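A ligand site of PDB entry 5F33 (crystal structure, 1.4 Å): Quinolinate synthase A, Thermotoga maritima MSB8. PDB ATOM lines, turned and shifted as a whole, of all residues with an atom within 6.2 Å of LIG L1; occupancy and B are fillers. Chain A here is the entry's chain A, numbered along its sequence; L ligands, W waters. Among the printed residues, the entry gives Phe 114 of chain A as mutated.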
ATOM      1  N   HIS A  26     -16.703 -20.070   1.957  1.00  0.00           N
ATOM      2  CA  HIS A  26     -15.435 -20.390   2.600  1.00  0.00           C
ATOM      3  C   HIS A  26     -14.720 -21.506   1.825  1.00  0.00           C
ATOM      4  O   HIS A  26     -15.329 -22.396   1.219  1.00  0.00           O
ATOM      5  CB  HIS A  26     -15.623 -20.709   4.085  1.00  0.00           C
ATOM      6  CG  HIS A  26     -14.328 -20.853   4.827  1.00  0.00           C
ATOM      7  ND1 HIS A  26     -13.701 -22.064   4.946  1.00  0.00           N
ATOM      8  CD2 HIS A  26     -13.506 -19.949   5.405  1.00  0.00           C
ATOM      9  CE1 HIS A  26     -12.564 -21.899   5.586  1.00  0.00           C
ATOM     10  NE2 HIS A  26     -12.419 -20.620   5.871  1.00  0.00           N
ATOM     11  N   ASN A  27     -13.401 -21.484   1.937  1.00  0.00           N
ATOM     12  CA  ASN A  27     -12.521 -22.491   1.347  1.00  0.00           C
ATOM     13  C   ASN A  27     -12.781 -23.947   1.755  1.00  0.00           C
ATOM     14  O   ASN A  27     -12.302 -24.844   1.071  1.00  0.00           O
ATOM     15  CB  ASN A  27     -11.071 -22.143   1.678  1.00  0.00           C
ATOM     16  CG  ASN A  27     -10.529 -20.943   0.897  1.00  0.00           C
ATOM     17  OD1 ASN A  27     -10.933 -20.703  -0.217  1.00  0.00           O
ATOM     18  ND2 ASN A  27      -9.594 -20.211   1.479  1.00  0.00           N
ATOM     19  N   TYR A  28     -13.517 -24.195   2.821  1.00  0.00           N
ATOM     20  CA  TYR A  28     -13.783 -25.574   3.250  1.00  0.00           C
ATOM     21  C   TYR A  28     -15.100 -26.086   2.713  1.00  0.00           C
ATOM     22  O   TYR A  28     -15.501 -27.208   3.019  1.00  0.00           O
ATOM     23  CB  TYR A  28     -13.757 -25.735   4.759  1.00  0.00           C
ATOM     24  CG  TYR A  28     -12.452 -25.393   5.455  1.00  0.00           C
ATOM     25  CD1 TYR A  28     -11.250 -25.282   4.752  1.00  0.00           C
ATOM     26  CD2 TYR A  28     -12.432 -25.143   6.827  1.00  0.00           C
ATOM     27  CE1 TYR A  28     -10.075 -24.986   5.402  1.00  0.00           C
ATOM     28  CE2 TYR A  28     -11.237 -24.837   7.477  1.00  0.00           C
ATOM     29  CZ  TYR A  28     -10.070 -24.739   6.755  1.00  0.00           C
ATOM     30  OH  TYR A  28      -8.907 -24.446   7.436  1.00  0.00           O
ATOM     31  N   GLY A  41     -13.084 -17.667  -0.346  1.00  0.00           N
ATOM     32  CA  GLY A  41     -11.881 -17.245   0.374  1.00  0.00           C
ATOM     33  C   GLY A  41     -11.830 -17.689   1.800  1.00  0.00           C
ATOM     34  O   GLY A  41     -12.666 -18.481   2.254  1.00  0.00           O
ATOM     35  N   ASP A  42     -10.805 -17.208   2.487  1.00  0.00           N
ATOM     36  CA  ASP A  42     -10.646 -17.507   3.900  1.00  0.00           C
ATOM     37  C   ASP A  42     -11.452 -16.533   4.747  1.00  0.00           C
ATOM     38  O   ASP A  42     -12.159 -15.649   4.199  1.00  0.00           O
ATOM     39  CB  ASP A  42      -9.183 -17.612   4.297  1.00  0.00           C
ATOM     40  CG  ASP A  42      -8.470 -16.306   4.471  1.00  0.00           C
ATOM     41  OD1 ASP A  42      -9.004 -15.219   4.239  1.00  0.00           O
ATOM     42  OD2 ASP A  42      -7.264 -16.383   4.897  1.00  0.00           O
ATOM     43  N   SER A  43     -11.393 -16.671   6.075  1.00  0.00           N
ATOM     44  CA  SER A  43     -12.305 -15.855   6.915  1.00  0.00           C
ATOM     45  C   SER A  43     -12.006 -14.373   6.765  1.00  0.00           C
ATOM     46  O   SER A  43     -12.952 -13.550   6.676  1.00  0.00           O
ATOM     47  CB  SER A  43     -12.231 -16.302   8.370  1.00  0.00           C
ATOM     48  OG  SER A  43     -12.653 -17.642   8.494  1.00  0.00           O
ATOM     49  N   LEU A  44     -10.735 -13.998   6.692  1.00  0.00           N
ATOM     50  CA  LEU A  44     -10.363 -12.588   6.560  1.00  0.00           C
ATOM     51  C   LEU A  44     -10.791 -12.047   5.208  1.00  0.00           C
ATOM     52  O   LEU A  44     -11.293 -10.920   5.115  1.00  0.00           O
ATOM     53  CB  LEU A  44      -8.870 -12.368   6.768  1.00  0.00           C
ATOM     54  CG  LEU A  44      -8.356 -10.909   6.650  1.00  0.00           C
ATOM     55  CD1 LEU A  44      -9.073 -10.028   7.664  1.00  0.00           C
ATOM     56  CD2 LEU A  44      -6.858 -10.860   6.867  1.00  0.00           C
ATOM     57  N   VAL A  63     -19.903 -21.357   7.997  1.00  0.00           N
ATOM     58  CA  VAL A  63     -20.520 -21.621   9.298  1.00  0.00           C
ATOM     59  C   VAL A  63     -21.067 -20.354   9.918  1.00  0.00           C
ATOM     60  O   VAL A  63     -20.709 -19.217   9.494  1.00  0.00           O
ATOM     61  CB  VAL A  63     -19.609 -22.334  10.270  1.00  0.00           C
ATOM     62  CG1 VAL A  63     -19.268 -23.737   9.767  1.00  0.00           C
ATOM     63  CG2 VAL A  63     -18.352 -21.498  10.542  1.00  0.00           C
ATOM     64  N   CYS A  88     -19.315 -23.728  14.302  1.00  0.00           N
ATOM     65  CA  CYS A  88     -17.993 -24.208  14.731  1.00  0.00           C
ATOM     66  C   CYS A  88     -18.087 -24.638  16.212  1.00  0.00           C
ATOM     67  O   CYS A  88     -18.321 -23.817  17.067  1.00  0.00           O
ATOM     68  CB  CYS A  88     -16.945 -23.118  14.571  1.00  0.00           C
ATOM     69  SG  CYS A  88     -15.335 -23.594  15.230  1.00  0.00           S
ATOM     70  N   PHE A 114     -10.885 -14.791  18.229  1.00  0.00           N
ATOM     71  CA  PHE A 114     -10.874 -15.433  16.933  1.00  0.00           C
ATOM     72  C   PHE A 114     -12.296 -15.346  16.375  1.00  0.00           C
ATOM     73  O   PHE A 114     -13.296 -15.375  17.101  1.00  0.00           O
ATOM     74  CB  PHE A 114     -10.366 -16.864  17.144  1.00  0.00           C
ATOM     75  CG  PHE A 114     -10.229 -17.698  15.902  1.00  0.00           C
ATOM     76  CD1 PHE A 114      -9.500 -17.241  14.798  1.00  0.00           C
ATOM     77  CD2 PHE A 114     -10.768 -18.986  15.861  1.00  0.00           C
ATOM     78  CE1 PHE A 114      -9.361 -18.026  13.676  1.00  0.00           C
ATOM     79  CE2 PHE A 114     -10.644 -19.774  14.720  1.00  0.00           C
ATOM     80  CZ  PHE A 114      -9.933 -19.292  13.627  1.00  0.00           C
ATOM     81  N   VAL A 115     -12.396 -15.288  15.058  1.00  0.00           N
ATOM     82  CA  VAL A 115     -13.655 -15.131  14.384  1.00  0.00           C
ATOM     83  C   VAL A 115     -14.674 -16.274  14.642  1.00  0.00           C
ATOM     84  O   VAL A 115     -15.888 -16.053  14.618  1.00  0.00           O
ATOM     85  CB  VAL A 115     -13.368 -14.879  12.885  1.00  0.00           C
ATOM     86  CG1 VAL A 115     -12.890 -16.136  12.177  1.00  0.00           C
ATOM     87  CG2 VAL A 115     -14.545 -14.259  12.232  1.00  0.00           C
ATOM     88  N   ASN A 116     -14.171 -17.484  14.945  1.00  0.00           N
ATOM     89  CA  ASN A 116     -15.044 -18.578  15.338  1.00  0.00           C
ATOM     90  C   ASN A 116     -15.415 -18.450  16.814  1.00  0.00           C
ATOM     91  O   ASN A 116     -14.859 -19.096  17.689  1.00  0.00           O
ATOM     92  CB  ASN A 116     -14.435 -19.930  14.965  1.00  0.00           C
ATOM     93  CG  ASN A 116     -14.367 -20.132  13.450  1.00  0.00           C
ATOM     94  OD1 ASN A 116     -14.851 -19.293  12.644  1.00  0.00           O
ATOM     95  ND2 ASN A 116     -13.754 -21.223  13.039  1.00  0.00           N
ATOM     96  N   THR A 130      -8.577 -13.177  12.695  1.00  0.00           N
ATOM     97  CA  THR A 130      -8.655 -14.458  12.017  1.00  0.00           C
ATOM     98  C   THR A 130      -7.270 -15.071  12.052  1.00  0.00           C
ATOM     99  O   THR A 130      -6.315 -14.463  12.513  1.00  0.00           O
ATOM    100  CB  THR A 130      -9.106 -14.338  10.533  1.00  0.00           C
ATOM    101  OG1 THR A 130      -7.988 -13.968   9.735  1.00  0.00           O
ATOM    102  CG2 THR A 130     -10.215 -13.323  10.381  1.00  0.00           C
ATOM    103  N   SER A 131      -7.144 -16.271  11.508  1.00  0.00           N
ATOM    104  CA  SER A 131      -5.865 -16.983  11.456  1.00  0.00           C
ATOM    105  C   SER A 131      -4.800 -16.191  10.714  1.00  0.00           C
ATOM    106  O   SER A 131      -3.612 -16.270  11.030  1.00  0.00           O
ATOM    107  CB  SER A 131      -6.066 -18.339  10.783  1.00  0.00           C
ATOM    108  OG  SER A 131      -7.245 -18.962  11.281  1.00  0.00           O
ATOM    109  N   ALA A 132      -5.233 -15.461   9.694  1.00  0.00           N
ATOM    110  CA  ALA A 132      -4.355 -14.691   8.848  1.00  0.00           C
ATOM    111  C   ALA A 132      -3.693 -13.510   9.544  1.00  0.00           C
ATOM    112  O   ALA A 132      -2.530 -13.233   9.294  1.00  0.00           O
ATOM    113  CB  ALA A 132      -5.123 -14.197   7.609  1.00  0.00           C
ATOM    114  N   CYS A 175      -9.420 -26.898  17.532  1.00  0.00           N
ATOM    115  CA  CYS A 175     -10.143 -27.348  16.344  1.00  0.00           C
ATOM    116  C   CYS A 175      -9.780 -28.809  16.159  1.00  0.00           C
ATOM    117  O   CYS A 175      -8.623 -29.094  15.845  1.00  0.00           O
ATOM    118  CB  CYS A 175      -9.717 -26.546  15.124  1.00  0.00           C
ATOM    119  SG  CYS A 175     -10.323 -27.321  13.589  1.00  0.00           S
ATOM    120  N   HIS A 178      -7.850 -29.890  12.779  1.00  0.00           N
ATOM    121  CA  HIS A 178      -6.444 -29.558  12.590  1.00  0.00           C
ATOM    122  C   HIS A 178      -5.492 -30.299  13.541  1.00  0.00           C
ATOM    123  O   HIS A 178      -4.277 -30.015  13.569  1.00  0.00           O
ATOM    124  CB  HIS A 178      -6.270 -28.047  12.716  1.00  0.00           C
ATOM    125  CG  HIS A 178      -6.727 -27.305  11.507  1.00  0.00           C
ATOM    126  ND1 HIS A 178      -7.996 -26.783  11.387  1.00  0.00           N
ATOM    127  CD2 HIS A 178      -6.106 -27.078  10.326  1.00  0.00           C
ATOM    128  CE1 HIS A 178      -8.113 -26.219  10.195  1.00  0.00           C
ATOM    129  NE2 HIS A 178      -6.974 -26.366   9.542  1.00  0.00           N
ATOM    130  N   HIS A 200      -1.850 -25.074   8.887  1.00  0.00           N
ATOM    131  CA  HIS A 200      -2.646 -24.015   9.494  1.00  0.00           C
ATOM    132  C   HIS A 200      -2.154 -23.708  10.890  1.00  0.00           C
ATOM    133  O   HIS A 200      -1.711 -24.618  11.567  1.00  0.00           O
ATOM    134  CB  HIS A 200      -4.084 -24.496   9.562  1.00  0.00           C
ATOM    135  CG  HIS A 200      -5.074 -23.388   9.637  1.00  0.00           C
ATOM    136  ND1 HIS A 200      -5.374 -22.759  10.823  1.00  0.00           N
ATOM    137  CD2 HIS A 200      -5.743 -22.728   8.665  1.00  0.00           C
ATOM    138  CE1 HIS A 200      -6.225 -21.785  10.582  1.00  0.00           C
ATOM    139  NE2 HIS A 200      -6.458 -21.747   9.289  1.00  0.00           N
ATOM    140  N   PRO A 201      -2.260 -22.438  11.364  1.00  0.00           N
ATOM    141  CA  PRO A 201      -1.835 -22.158  12.741  1.00  0.00           C
ATOM    142  C   PRO A 201      -2.698 -22.778  13.839  1.00  0.00           C
ATOM    143  O   PRO A 201      -2.276 -22.813  14.994  1.00  0.00           O
ATOM    144  CB  PRO A 201      -1.844 -20.647  12.824  1.00  0.00           C
ATOM    145  CG  PRO A 201      -2.746 -20.218  11.729  1.00  0.00           C
ATOM    146  CD  PRO A 201      -2.518 -21.195  10.622  1.00  0.00           C
ATOM    147  N   GLU A 202      -3.858 -23.320  13.476  1.00  0.00           N
ATOM    148  CA  GLU A 202      -4.731 -24.069  14.392  1.00  0.00           C
ATOM    149  C   GLU A 202      -4.162 -25.467  14.681  1.00  0.00           C
ATOM    150  O   GLU A 202      -4.657 -26.155  15.574  1.00  0.00           O
ATOM    151  CB  GLU A 202      -6.164 -24.214  13.823  1.00  0.00           C
ATOM    152  CG  GLU A 202      -6.987 -22.930  13.892  1.00  0.00           C
ATOM    153  CD  GLU A 202      -8.239 -22.985  13.047  1.00  0.00           C
ATOM    154  OE1 GLU A 202      -8.801 -24.080  12.808  1.00  0.00           O
ATOM    155  OE2 GLU A 202      -8.660 -21.929  12.570  1.00  0.00           O
ATOM    156  N   GLY A 215       0.213 -20.815   7.915  1.00  0.00           N
ATOM    157  CA  GLY A 215      -0.653 -19.699   7.634  1.00  0.00           C
ATOM    158  C   GLY A 215      -2.108 -20.078   7.414  1.00  0.00           C
ATOM    159  O   GLY A 215      -2.459 -21.264   7.327  1.00  0.00           O
ATOM    160  N   SER A 216      -2.942 -19.052   7.342  1.00  0.00           N
ATOM    161  CA  SER A 216      -4.357 -19.206   7.042  1.00  0.00           C
ATOM    162  C   SER A 216      -4.513 -19.858   5.671  1.00  0.00           C
ATOM    163  O   SER A 216      -3.609 -19.826   4.868  1.00  0.00           O
ATOM    164  CB  SER A 216      -5.045 -17.857   7.007  1.00  0.00           C
ATOM    165  OG  SER A 216      -4.635 -17.102   5.867  1.00  0.00           O
ATOM    166  N   THR A 217      -5.730 -20.253   5.342  1.00  0.00           N
ATOM    167  CA  THR A 217      -5.964 -20.828   4.035  1.00  0.00           C
ATOM    168  C   THR A 217      -5.725 -19.790   2.924  1.00  0.00           C
ATOM    169  O   THR A 217      -5.211 -20.127   1.892  1.00  0.00           O
ATOM    170  CB  THR A 217      -7.328 -21.493   3.929  1.00  0.00           C
ATOM    171  OG1 THR A 217      -8.360 -20.524   4.084  1.00  0.00           O
ATOM    172  CG2 THR A 217      -7.486 -22.585   4.997  1.00  0.00           C
ATOM    173  N   GLY A 218      -6.006 -18.516   3.174  1.00  0.00           N
ATOM    174  CA  GLY A 218      -5.714 -17.513   2.151  1.00  0.00           C
ATOM    175  C   GLY A 218      -4.219 -17.336   1.948  1.00  0.00           C
ATOM    176  O   GLY A 218      -3.774 -17.123   0.823  1.00  0.00           O
ATOM    177  N   THR A 236      -4.513 -28.808   6.392  1.00  0.00           N
ATOM    178  CA  THR A 236      -5.767 -28.132   6.753  1.00  0.00           C
ATOM    179  C   THR A 236      -6.905 -28.992   6.257  1.00  0.00           C
ATOM    180  O   THR A 236      -6.700 -30.135   5.830  1.00  0.00           O
ATOM    181  CB  THR A 236      -5.817 -26.664   6.236  1.00  0.00           C
ATOM    182  OG1 THR A 236      -6.860 -25.980   6.919  1.00  0.00           O
ATOM    183  CG2 THR A 236      -6.055 -26.602   4.714  1.00  0.00           C
ATOM    184  N   MET A 264     -18.797 -27.785   8.057  1.00  0.00           N
ATOM    185  CA  MET A 264     -18.619 -27.168   6.735  1.00  0.00           C
ATOM    186  C   MET A 264     -19.246 -27.982   5.620  1.00  0.00           C
ATOM    187  O   MET A 264     -19.662 -27.408   4.619  1.00  0.00           O
ATOM    188  CB  MET A 264     -17.128 -26.955   6.452  1.00  0.00           C
ATOM    189  CG  MET A 264     -16.508 -25.828   7.269  1.00  0.00           C
ATOM    190  SD  MET A 264     -16.964 -24.235   6.568  1.00  0.00           S
ATOM    191  CE  MET A 264     -15.886 -23.207   7.577  1.00  0.00           C
HETATM  192  C1  LIG L   1     -10.825 -22.390   9.882  1.00  0.00           C
HETATM  193  C2  LIG L   1      -9.711 -21.789   9.056  1.00  0.00           C
HETATM  194  N1  LIG L   1     -12.011 -21.803   9.830  1.00  0.00           N
HETATM  195  O1  LIG L   1     -13.128 -22.357  10.436  1.00  0.00           O
HETATM  196  O2  LIG L   1     -10.602 -23.444  10.497  1.00  0.00           O
HETATM  197  O3  LIG L   1      -9.657 -20.371   8.945  1.00  0.00           O
HETATM  198  O4  LIG L   1      -7.674 -19.892   7.526  1.00  0.00           O
HETATM  199  O5  LIG L   1      -9.964 -19.991   6.438  1.00  0.00           O
HETATM  200  O6  LIG L   1      -9.480 -18.159   8.006  1.00  0.00           O
HETATM  201  P1  LIG L   1      -9.132 -19.577   7.632  1.00  0.00           P
HETATM  202 FE1  LG2 L   2     -12.233 -26.333  12.845  1.00  0.00          FE
HETATM  203 FE2  LG2 L   2     -14.594 -26.534  11.417  1.00  0.00          FE
HETATM  204 FE3  LG2 L   2     -12.804 -24.173  11.251  1.00  0.00          FE
HETATM  205 FE4  LG2 L   2     -14.399 -24.789  13.515  1.00  0.00          FE
HETATM  206  S1  LG2 L   2     -15.249 -24.351  11.488  1.00  0.00           S
HETATM  207  S2  LG2 L   2     -12.120 -24.149  13.438  1.00  0.00           S
HETATM  208  S3  LG2 L   2     -14.290 -27.134  13.623  1.00  0.00           S
HETATM  209  S4  LG2 L   2     -12.456 -26.437  10.610  1.00  0.00           S
HETATM  210  O   HOH W   1     -12.076 -18.980  10.625  1.00  0.00           O
HETATM  211  O   HOH W   2      -8.298 -15.828   7.591  1.00  0.00           O
HETATM  212  O   HOH W   3     -15.210 -19.824   9.641  1.00  0.00           O
HETATM  213  O   HOH W   4      -9.493 -17.593  10.452  1.00  0.00           O
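A ring nitrogen (NE2) of His 26 sits at hydrogen-bond distance from an oxygen (O5) of LIG L1 (2.6 Å). A ring nitrogen (NE2) of His 200 lies within hydrogen-bond range of an oxygen (O4) of LIG L1, 2.8 Å away. An oxygen (O4) of LIG L1 sits at hydrogen-bond distance from the backbone NH (N) of Thr 217. OG1 of Thr 217 sits at hydrogen-bond distance from O5 of LIG L1, at 2.9 Å. An oxygen (O1) of LIG L1 lies close to the side-chain amide nitrogen (ND2) of Asn 116, 2.9 Å away. The backbone NH (N) of Ser 43 is in hydrogen-bond range of an oxygen (O6) of LIG L1. An oxygen (O6) of LIG L1 sits at hydrogen-bond distance from the side-chain hydroxyl of Ser 43, at 3.3 Å. A sulfur (S2) of LG2 L2 sits close to the side-chain amide nitrogen (ND2) of Asn 116 (3.4 Å). An iron atom (FE1) of LG2 L2 is bound by the side-chain sulfur (SG) of Cys 175. SG of Cys 88 is bound to FE4 of LG2 L2, 2.3 Å away.
O1 of LIG L1 binds FE3 of LG2 L2 (2.0 Å).
ND1 of His 200 is in hydrogen-bond range of N of Glu 202, at 3.1 Å. The side-chain hydroxyl (OG1) of Thr 217 sits at hydrogen-bond distance from the side-chain amide nitrogen (ND2) of Asn 27. The side-chain amide nitrogen (ND2) of Asn 116 sits close to the side-chain sulfur (SG) of Cys 88 (3.6 Å). ND1 of His 178 lies within hydrogen-bond range of OE1 of Glu 202, at 3.2 Å. The side-chain hydroxyl (OH) of Tyr 28 lies close to a ring nitrogen (NE2) of His 178, 3.4 Å away. OD1 of Asp 42 sits at hydrogen-bond distance from N of Leu 44 (3.2 Å). The backbone NH of Gly 218 is in hydrogen-bond range of the side-chain carboxylate of Asp 42. A ring nitrogen (ND1) of His 178 sits close to the side-chain sulfur (SG) of Cys 175 (3.2 Å).
OE1 of Glu 202 lies close to O2 of LIG L1, at 3.0 Å. Tyr 28 touches LIG L1 (OH to C2, 3.2 Å). Asp 42 touches LIG L1. OG of Ser 131 touches O3 of LIG L1, 3.6 Å away. His 178 touches LIG L1. Ser 216 touches LIG L1 (CB to O4, 3.4 Å). Hydrophobic or aromatic side chains within 4 Å of LIG L1: His 26, Tyr 28, His 178 and His 200. Of the 26 residues printed, 11 come within 4 Å of LIG L1.
Water W4 lies within hydrogen-bond range of an oxygen (O6) of LIG L1 (2.5 Å) and the side-chain hydroxyl of Ser 131 (2.8 Å). Water W2 lies within hydrogen-bond range of O6 of LIG L1, OG1 of Thr 130, OD2 of Asp 42 and N of Leu 44. Water W1 lies within hydrogen-bond range of the side-chain hydroxyl of Ser 43, a nitrogen (N1) of LIG L1 and the side-chain amide oxygen of Asn 116.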
